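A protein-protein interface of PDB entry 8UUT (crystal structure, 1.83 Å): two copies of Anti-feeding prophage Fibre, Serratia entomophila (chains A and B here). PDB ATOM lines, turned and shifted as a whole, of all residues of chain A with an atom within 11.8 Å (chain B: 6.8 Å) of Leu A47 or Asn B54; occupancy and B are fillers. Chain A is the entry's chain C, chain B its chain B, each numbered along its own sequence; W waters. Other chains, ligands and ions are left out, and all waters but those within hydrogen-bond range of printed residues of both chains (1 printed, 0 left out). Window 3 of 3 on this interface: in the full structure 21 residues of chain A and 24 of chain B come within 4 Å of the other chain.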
ATOM      1  N   ASN A  43      19.117 -17.532  13.894  1.00  0.00           N
ATOM      2  CA  ASN A  43      18.401 -16.503  13.147  1.00  0.00           C
ATOM      3  C   ASN A  43      18.297 -15.204  13.962  1.00  0.00           C
ATOM      4  O   ASN A  43      17.901 -14.164  13.422  1.00  0.00           O
ATOM      5  CB  ASN A  43      17.008 -17.000  12.744  1.00  0.00           C
ATOM      6  N   GLY A  44      18.662 -15.270  15.250  1.00  0.00           N
ATOM      7  CA  GLY A  44      18.655 -14.117  16.139  1.00  0.00           C
ATOM      8  C   GLY A  44      17.284 -13.607  16.528  1.00  0.00           C
ATOM      9  O   GLY A  44      17.181 -12.681  17.343  1.00  0.00           O
ATOM     10  N   VAL A  45      16.226 -14.177  15.972  1.00  0.00           N
ATOM     11  CA  VAL A  45      14.864 -13.766  16.263  1.00  0.00           C
ATOM     12  C   VAL A  45      14.009 -15.000  16.045  1.00  0.00           C
ATOM     13  O   VAL A  45      14.371 -15.883  15.265  1.00  0.00           O
ATOM     14  CB  VAL A  45      14.442 -12.582  15.364  1.00  0.00           C
ATOM     15  CG1 VAL A  45      14.582 -12.964  13.895  1.00  0.00           C
ATOM     16  CG2 VAL A  45      13.040 -12.120  15.681  1.00  0.00           C
ATOM     17  N   GLY A  46      12.904 -15.090  16.765  1.00  0.00           N
ATOM     18  CA  GLY A  46      12.073 -16.278  16.687  1.00  0.00           C
ATOM     19  C   GLY A  46      10.616 -15.936  16.870  1.00  0.00           C
ATOM     20  O   GLY A  46      10.266 -14.953  17.533  1.00  0.00           O
ATOM     21  N   LEU A  47       9.759 -16.743  16.252  1.00  0.00           N
ATOM     22  CA  LEU A  47       8.334 -16.679  16.546  1.00  0.00           C
ATOM     23  C   LEU A  47       8.076 -17.323  17.900  1.00  0.00           C
ATOM     24  O   LEU A  47       8.600 -18.399  18.194  1.00  0.00           O
ATOM     25  CB  LEU A  47       7.538 -17.401  15.459  1.00  0.00           C
ATOM     26  CG  LEU A  47       7.514 -16.737  14.090  1.00  0.00           C
ATOM     27  CD1 LEU A  47       6.848 -17.665  13.071  1.00  0.00           C
ATOM     28  CD2 LEU A  47       6.770 -15.438  14.178  1.00  0.00           C
ATOM     29  N   LYS A  48       7.281 -16.667  18.731  1.00  0.00           N
ATOM     30  CA  LYS A  48       6.844 -17.334  19.944  1.00  0.00           C
ATOM     31  C   LYS A  48       5.944 -18.513  19.588  1.00  0.00           C
ATOM     32  O   LYS A  48       5.328 -18.558  18.518  1.00  0.00           O
ATOM     33  CB  LYS A  48       6.108 -16.362  20.860  1.00  0.00           C
ATOM     34  CG  LYS A  48       6.922 -15.134  21.268  1.00  0.00           C
ATOM     35  CD  LYS A  48       8.211 -15.537  21.963  1.00  0.00           C
ATOM     36  CE  LYS A  48       8.892 -14.324  22.581  1.00  0.00           C
ATOM     37  NZ  LYS A  48       8.900 -14.374  24.075  1.00  0.00           N
ATOM     38  N   SER A  49       5.885 -19.481  20.502  1.00  0.00           N
ATOM     39  CA  SER A  49       5.101 -20.687  20.255  1.00  0.00           C
ATOM     40  C   SER A  49       3.630 -20.367  20.037  1.00  0.00           C
ATOM     41  O   SER A  49       2.940 -21.097  19.321  1.00  0.00           O
ATOM     42  CB  SER A  49       5.251 -21.653  21.426  1.00  0.00           C
ATOM     43  OG  SER A  49       4.620 -21.108  22.570  1.00  0.00           O
ATOM     44  N   THR A  50       3.135 -19.288  20.646  1.00  0.00           N
ATOM     45  CA  THR A  50       1.752 -18.858  20.502  1.00  0.00           C
ATOM     46  C   THR A  50       1.596 -17.746  19.469  1.00  0.00           C
ATOM     47  O   THR A  50       0.620 -16.993  19.521  1.00  0.00           O
ATOM     48  CB  THR A  50       1.184 -18.416  21.857  1.00  0.00           C
ATOM     49  OG1 THR A  50       1.992 -17.369  22.410  1.00  0.00           O
ATOM     50  CG2 THR A  50       1.130 -19.590  22.832  1.00  0.00           C
ATOM     51  N   ALA A  51       2.533 -17.631  18.520  1.00  0.00           N
ATOM     52  CA  ALA A  51       2.398 -16.601  17.492  1.00  0.00           C
ATOM     53  C   ALA A  51       1.082 -16.736  16.737  1.00  0.00           C
ATOM     54  O   ALA A  51       0.540 -15.738  16.251  1.00  0.00           O
ATOM     55  CB  ALA A  51       3.573 -16.668  16.513  1.00  0.00           C
ATOM     56  N   TRP A  52       0.549 -17.959  16.633  1.00  0.00           N
ATOM     57  CA  TRP A  52      -0.716 -18.159  15.935  1.00  0.00           C
ATOM     58  C   TRP A  52      -1.846 -17.343  16.558  1.00  0.00           C
ATOM     59  O   TRP A  52      -2.746 -16.894  15.841  1.00  0.00           O
ATOM     60  CB  TRP A  52      -1.071 -19.652  15.905  1.00  0.00           C
ATOM     61  CG  TRP A  52      -1.141 -20.296  17.266  1.00  0.00           C
ATOM     62  CD1 TRP A  52      -0.119 -20.890  17.940  1.00  0.00           C
ATOM     63  CD2 TRP A  52      -2.301 -20.422  18.101  1.00  0.00           C
ATOM     64  NE1 TRP A  52      -0.564 -21.370  19.153  1.00  0.00           N
ATOM     65  CE2 TRP A  52      -1.901 -21.098  19.272  1.00  0.00           C
ATOM     66  CE3 TRP A  52      -3.635 -20.029  17.975  1.00  0.00           C
ATOM     67  CZ2 TRP A  52      -2.790 -21.387  20.310  1.00  0.00           C
ATOM     68  CZ3 TRP A  52      -4.521 -20.310  19.019  1.00  0.00           C
ATOM     69  CH2 TRP A  52      -4.091 -20.979  20.167  1.00  0.00           C
ATOM     70  N   ILE A  53      -1.812 -17.115  17.876  1.00  0.00           N
ATOM     71  CA  ILE A  53      -2.854 -16.300  18.504  1.00  0.00           C
ATOM     72  C   ILE A  53      -2.845 -14.890  17.925  1.00  0.00           C
ATOM     73  O   ILE A  53      -3.881 -14.351  17.519  1.00  0.00           O
ATOM     74  CB  ILE A  53      -2.668 -16.261  20.031  1.00  0.00           C
ATOM     75  CG1 ILE A  53      -2.853 -17.653  20.655  1.00  0.00           C
ATOM     76  CG2 ILE A  53      -3.636 -15.252  20.629  1.00  0.00           C
ATOM     77  CD1 ILE A  53      -2.433 -17.722  22.106  1.00  0.00           C
ATOM     78  N   ASN A  54      -1.666 -14.265  17.914  1.00  0.00           N
ATOM     79  CA  ASN A  54      -1.510 -12.941  17.324  1.00  0.00           C
ATOM     80  C   ASN A  54      -1.979 -12.928  15.882  1.00  0.00           C
ATOM     81  O   ASN A  54      -2.738 -12.041  15.465  1.00  0.00           O
ATOM     82  CB  ASN A  54      -0.046 -12.526  17.408  1.00  0.00           C
ATOM     83  CG  ASN A  54       0.471 -12.537  18.816  1.00  0.00           C
ATOM     84  OD1 ASN A  54       0.783 -13.598  19.358  1.00  0.00           O
ATOM     85  ND2 ASN A  54       0.579 -11.347  19.427  1.00  0.00           N
ATOM     86  N   VAL A  55      -1.543 -13.928  15.106  1.00  0.00           N
ATOM     87  CA  VAL A  55      -1.856 -13.962  13.681  1.00  0.00           C
ATOM     88  C   VAL A  55      -3.362 -14.064  13.465  1.00  0.00           C
ATOM     89  O   VAL A  55      -3.956 -13.269  12.726  1.00  0.00           O
ATOM     90  CB  VAL A  55      -1.110 -15.123  13.002  1.00  0.00           C
ATOM     91  CG1 VAL A  55      -1.596 -15.307  11.560  1.00  0.00           C
ATOM     92  CG2 VAL A  55       0.382 -14.874  13.032  1.00  0.00           C
ATOM     93  N   MET A  56      -4.001 -15.053  14.104  1.00  0.00           N
ATOM     94  CA  MET A  56      -5.424 -15.319  13.881  1.00  0.00           C
ATOM     95  C   MET A  56      -6.324 -14.249  14.494  1.00  0.00           C
ATOM     96  O   MET A  56      -7.404 -13.986  13.957  1.00  0.00           O
ATOM     97  CB  MET A  56      -5.794 -16.694  14.448  1.00  0.00           C
ATOM     98  CG  MET A  56      -5.021 -17.882  13.882  1.00  0.00           C
ATOM     99  SD  MET A  56      -4.944 -17.934  12.076  1.00  0.00           S
ATOM    100  CE  MET A  56      -6.676 -18.243  11.751  1.00  0.00           C
ATOM    101  N   ARG A  89      -7.878 -28.267  17.191  1.00  0.00           N
ATOM    102  CA  ARG A  89      -6.469 -28.450  17.528  1.00  0.00           C
ATOM    103  C   ARG A  89      -6.271 -29.858  18.068  1.00  0.00           C
ATOM    104  O   ARG A  89      -7.193 -30.461  18.626  1.00  0.00           O
ATOM    105  CB  ARG A  89      -5.964 -27.449  18.598  1.00  0.00           C
ATOM    106  CG  ARG A  89      -6.275 -25.968  18.362  1.00  0.00           C
ATOM    107  CD  ARG A  89      -5.596 -25.104  19.424  1.00  0.00           C
ATOM    108  NE  ARG A  89      -4.169 -24.919  19.150  1.00  0.00           N
ATOM    109  CZ  ARG A  89      -3.187 -25.035  20.040  1.00  0.00           C
ATOM    110  NH1 ARG A  89      -3.440 -25.390  21.296  1.00  0.00           N
ATOM    111  NH2 ARG A  89      -1.933 -24.803  19.662  1.00  0.00           N
ATOM    112  N   LEU B  47       9.600 -12.105   7.909  1.00  0.00           N
ATOM    113  CA  LEU B  47       9.065 -13.459   7.937  1.00  0.00           C
ATOM    114  C   LEU B  47       9.686 -14.259   6.793  1.00  0.00           C
ATOM    115  O   LEU B  47       9.840 -13.745   5.680  1.00  0.00           O
ATOM    116  CB  LEU B  47       7.542 -13.393   7.786  1.00  0.00           C
ATOM    117  CG  LEU B  47       6.776 -12.693   8.921  1.00  0.00           C
ATOM    118  CD1 LEU B  47       5.325 -12.396   8.528  1.00  0.00           C
ATOM    119  CD2 LEU B  47       6.831 -13.523  10.205  1.00  0.00           C
ATOM    120  N   LYS B  48      10.061 -15.514   7.057  1.00  0.00           N
ATOM    121  CA  LYS B  48      10.436 -16.381   5.956  1.00  0.00           C
ATOM    122  C   LYS B  48       9.220 -16.575   5.043  1.00  0.00           C
ATOM    123  O   LYS B  48       8.065 -16.425   5.461  1.00  0.00           O
ATOM    124  CB  LYS B  48      10.892 -17.747   6.453  1.00  0.00           C
ATOM    125  CG  LYS B  48      12.090 -17.838   7.418  1.00  0.00           C
ATOM    126  CD  LYS B  48      13.538 -17.522   6.966  1.00  0.00           C
ATOM    127  CE  LYS B  48      13.852 -16.043   7.304  1.00  0.00           C
ATOM    128  NZ  LYS B  48      15.260 -15.622   7.051  1.00  0.00           N
ATOM    129  N   THR B  50       8.021 -19.252   4.097  1.00  0.00           N
ATOM    130  CA  THR B  50       7.271 -20.383   4.629  1.00  0.00           C
ATOM    131  C   THR B  50       6.836 -20.174   6.077  1.00  0.00           C
ATOM    132  O   THR B  50       6.609 -21.147   6.800  1.00  0.00           O
ATOM    133  CB  THR B  50       8.096 -21.662   4.506  1.00  0.00           C
ATOM    134  OG1 THR B  50       9.283 -21.542   5.305  1.00  0.00           O
ATOM    135  CG2 THR B  50       8.471 -21.930   3.053  1.00  0.00           C
ATOM    136  N   ALA B  51       6.702 -18.918   6.519  1.00  0.00           N
ATOM    137  CA  ALA B  51       6.246 -18.665   7.879  1.00  0.00           C
ATOM    138  C   ALA B  51       4.879 -19.288   8.133  1.00  0.00           C
ATOM    139  O   ALA B  51       4.584 -19.698   9.262  1.00  0.00           O
ATOM    140  CB  ALA B  51       6.205 -17.156   8.150  1.00  0.00           C
ATOM    141  N   TRP B  52       4.046 -19.399   7.091  1.00  0.00           N
ATOM    142  CA  TRP B  52       2.727 -20.007   7.267  1.00  0.00           C
ATOM    143  C   TRP B  52       2.821 -21.428   7.806  1.00  0.00           C
ATOM    144  O   TRP B  52       1.916 -21.880   8.516  1.00  0.00           O
ATOM    145  CB  TRP B  52       1.967 -19.972   5.946  1.00  0.00           C
ATOM    146  CG  TRP B  52       2.695 -20.656   4.824  1.00  0.00           C
ATOM    147  CD1 TRP B  52       3.558 -20.083   3.936  1.00  0.00           C
ATOM    148  CD2 TRP B  52       2.586 -22.036   4.448  1.00  0.00           C
ATOM    149  NE1 TRP B  52       4.014 -21.029   3.040  1.00  0.00           N
ATOM    150  CE2 TRP B  52       3.424 -22.232   3.330  1.00  0.00           C
ATOM    151  CE3 TRP B  52       1.857 -23.126   4.947  1.00  0.00           C
ATOM    152  CZ2 TRP B  52       3.559 -23.473   2.707  1.00  0.00           C
ATOM    153  CZ3 TRP B  52       1.996 -24.358   4.329  1.00  0.00           C
ATOM    154  CH2 TRP B  52       2.839 -24.518   3.218  1.00  0.00           C
ATOM    155  N   ILE B  53       3.915 -22.140   7.513  1.00  0.00           N
ATOM    156  CA  ILE B  53       4.104 -23.473   8.082  1.00  0.00           C
ATOM    157  C   ILE B  53       4.202 -23.401   9.600  1.00  0.00           C
ATOM    158  O   ILE B  53       3.526 -24.144  10.316  1.00  0.00           O
ATOM    159  CB  ILE B  53       5.346 -24.148   7.486  1.00  0.00           C
ATOM    160  CG1 ILE B  53       5.138 -24.445   5.998  1.00  0.00           C
ATOM    161  CG2 ILE B  53       5.647 -25.429   8.247  1.00  0.00           C
ATOM    162  CD1 ILE B  53       6.413 -24.931   5.303  1.00  0.00           C
ATOM    163  N   ASN B  54       5.072 -22.525  10.109  1.00  0.00           N
ATOM    164  CA  ASN B  54       5.211 -22.368  11.557  1.00  0.00           C
ATOM    165  C   ASN B  54       3.893 -21.964  12.192  1.00  0.00           C
ATOM    166  O   ASN B  54       3.517 -22.482  13.251  1.00  0.00           O
ATOM    167  CB  ASN B  54       6.271 -21.313  11.883  1.00  0.00           C
ATOM    168  CG  ASN B  54       7.604 -21.634  11.275  1.00  0.00           C
ATOM    169  OD1 ASN B  54       7.774 -21.504  10.064  1.00  0.00           O
ATOM    170  ND2 ASN B  54       8.557 -22.073  12.096  1.00  0.00           N
ATOM    171  N   VAL B  55       3.192 -21.015  11.574  1.00  0.00           N
ATOM    172  CA  VAL B  55       1.987 -20.463  12.183  1.00  0.00           C
ATOM    173  C   VAL B  55       0.879 -21.509  12.218  1.00  0.00           C
ATOM    174  O   VAL B  55       0.228 -21.714  13.250  1.00  0.00           O
ATOM    175  CB  VAL B  55       1.546 -19.193  11.430  1.00  0.00           C
ATOM    176  CG1 VAL B  55       0.202 -18.692  11.958  1.00  0.00           C
ATOM    177  CG2 VAL B  55       2.616 -18.099  11.538  1.00  0.00           C
ATOM    178  N   MET B  56       0.660 -22.198  11.092  1.00  0.00           N
ATOM    179  CA  MET B  56      -0.434 -23.161  11.010  1.00  0.00           C
ATOM    180  C   MET B  56      -0.159 -24.397  11.865  1.00  0.00           C
ATOM    181  O   MET B  56      -1.079 -24.938  12.486  1.00  0.00           O
ATOM    182  CB  MET B  56      -0.657 -23.543   9.551  1.00  0.00           C
ATOM    183  CG  MET B  56      -1.203 -22.431   8.648  1.00  0.00           C
ATOM    184  SD  MET B  56      -2.408 -21.298   9.380  1.00  0.00           S
ATOM    185  CE  MET B  56      -3.860 -22.309   9.129  1.00  0.00           C
ATOM    186  N   CYS B  57       1.101 -24.859  11.925  1.00  0.00           N
ATOM    187  CA  CYS B  57       1.437 -25.925  12.871  1.00  0.00           C
ATOM    188  C   CYS B  57       1.139 -25.507  14.304  1.00  0.00           C
ATOM    189  O   CYS B  57       0.639 -26.311  15.108  1.00  0.00           O
ATOM    190  CB  CYS B  57       2.905 -26.332  12.751  1.00  0.00           C
ATOM    191  SG  CYS B  57       3.361 -27.310  11.302  1.00  0.00           S
ATOM    192  N   GLY B  58       1.451 -24.259  14.653  1.00  0.00           N
ATOM    193  CA  GLY B  58       1.084 -23.771  15.971  1.00  0.00           C
ATOM    194  C   GLY B  58      -0.419 -23.712  16.157  1.00  0.00           C
ATOM    195  O   GLY B  58      -0.952 -24.158  17.182  1.00  0.00           O
ATOM    196  N   LEU B  59      -1.127 -23.176  15.153  1.00  0.00           N
ATOM    197  CA  LEU B  59      -2.578 -23.012  15.236  1.00  0.00           C
ATOM    198  C   LEU B  59      -3.290 -24.319  15.563  1.00  0.00           C
ATOM    199  O   LEU B  59      -4.202 -24.348  16.395  1.00  0.00           O
ATOM    200  CB  LEU B  59      -3.115 -22.454  13.917  1.00  0.00           C
ATOM    201  CG  LEU B  59      -4.638 -22.417  13.803  1.00  0.00           C
ATOM    202  CD1 LEU B  59      -5.204 -21.484  14.856  1.00  0.00           C
ATOM    203  CD2 LEU B  59      -5.061 -22.009  12.395  1.00  0.00           C
ATOM    204  N   PHE B  74      -1.941 -30.261   8.040  1.00  0.00           N
ATOM    205  CA  PHE B  74      -1.267 -30.204   9.333  1.00  0.00           C
ATOM    206  C   PHE B  74      -1.821 -31.312  10.218  1.00  0.00           C
ATOM    207  O   PHE B  74      -3.025 -31.339  10.496  1.00  0.00           O
ATOM    208  CB  PHE B  74      -1.459 -28.812   9.942  1.00  0.00           C
ATOM    209  CG  PHE B  74      -1.020 -27.731   9.009  1.00  0.00           C
ATOM    210  CD1 PHE B  74       0.324 -27.421   8.886  1.00  0.00           C
ATOM    211  CD2 PHE B  74      -1.929 -27.100   8.178  1.00  0.00           C
ATOM    212  CE1 PHE B  74       0.748 -26.458   7.974  1.00  0.00           C
ATOM    213  CE2 PHE B  74      -1.507 -26.145   7.266  1.00  0.00           C
ATOM    214  CZ  PHE B  74      -0.163 -25.829   7.169  1.00  0.00           C
ATOM    215  N   PRO B 161       8.228 -27.649  12.502  1.00  0.00           N
ATOM    216  CA  PRO B 161       9.418 -26.919  12.948  1.00  0.00           C
ATOM    217  C   PRO B 161       9.400 -26.630  14.448  1.00  0.00           C
ATOM    218  O   PRO B 161       8.357 -26.674  15.109  1.00  0.00           O
ATOM    219  CB  PRO B 161       9.356 -25.627  12.130  1.00  0.00           C
ATOM    220  CG  PRO B 161       7.887 -25.431  11.864  1.00  0.00           C
ATOM    221  CD  PRO B 161       7.347 -26.816  11.663  1.00  0.00           C
ATOM    222  OXT PRO B 161      10.449 -26.348  15.044  1.00  0.00           O
HETATM  223  O   HOH W   1       2.359 -20.491  15.793  1.00  0.00           O
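Leu A47 touches Asn B54, but with the chains exchanged Asn A54 does not touch Leu B47 (10.0 Å).
Trp A52 touches Val B55, but with the chains exchanged Val A55 does not touch Trp B52 (7.7 Å).
Val B55 touches its own counterpart, Val A55.
9 positions are printed for both chains.
Of the 8 pairs that touch across the chains among the printed residues, 1 has its exchanged pair printed and touching as well.
Hydrophobic or aromatic side chains of chain B that line the printed part of chain A: Val B55 and Leu B59.
Hydrophobic or aromatic side chains of chain A that line the printed part of chain B: Leu A47, Trp A52, Val A55 and Met A56.
The side-chain amide oxygen (OD1) of Asn B54 lies close to the backbone carbonyl oxygen (O) of Thr B50 (3.5 Å).
Asn B54 touches Leu A47 (CB to CD1, 3.9 Å).
Val B55 touches Trp A52 (O to CB, 3.6 Å).
Leu B59 touches Trp A52 (N to CG, 3.6 Å).
Val A55 touches Val B55 (CG1 to CG1, 3.9 Å).
CD1 of Leu B59 touches CG of Met A56 (3.7 Å).
Water W1 bridges the backbone NH of Trp A52 and the backbone carbonyl oxygen of Asn B54.
Of chain B, only Asn B54 (3.9 Å) comes within 4 Å of Leu A47.
Ser A49 touches none of the printed residues of chain B.
Of the printed residues of chain B, Trp A52 touches Val B55, Gly B58 and Leu B59.
Ile A53 touches none of the printed residues of chain B.
Printed residues of chain B within 4 Å of Met A56: Leu B59.
Printed residues of chain B within 4 Å of Arg A89: Gly B58 (2.7 Å) and Leu B59 (2.8 Å).
No residue of chain A comes within 4 Å of Thr B50.
No residue of chain A comes within 4 Å of Ala B51.
No residue of chain A comes within 4 Å of Trp B52.
No residue of chain A comes within 4 Å of Ile B53.
Of the printed residues of chain A, Asn B54 touches Leu A47 (3.9 Å).
No residue of chain A comes within 4 Å of Cys B57.
Of chain A, only Trp A52 (3.4 Å) and Arg A89 (2.7 Å) come within 4 Å of Gly B58.
Printed residues of chain A within 4 Å of Leu B59: Trp A52 (3.6 Å), Met A56 (3.7 Å) and Arg A89 (2.8 Å).
No residue of chain A comes within 4 Å of Pro B161.
The nearest residue of chain B that does not touch Leu A47 is Leu B47 (4.4 Å).
The nearest residue of chain A that does not touch Asn B54 is Trp A52 (6.0 Å).
The nearest printed residue of chain B that does not touch Trp A52 is Met B56 (5.7 Å).
The backbone carbonyl oxygen (O) of Leu B59 lies within hydrogen-bond range of the guanidinium group (NE) of Arg A89, at 2.8 Å.
The backbone carbonyl oxygen of Gly B58 lies within hydrogen-bond range of the indole nitrogen of Trp A52 (3.4 Å).
The guanidinium group of Arg A89 lies within hydrogen-bond range of the backbone carbonyl oxygen of Gly B58, 2.7 Å away.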
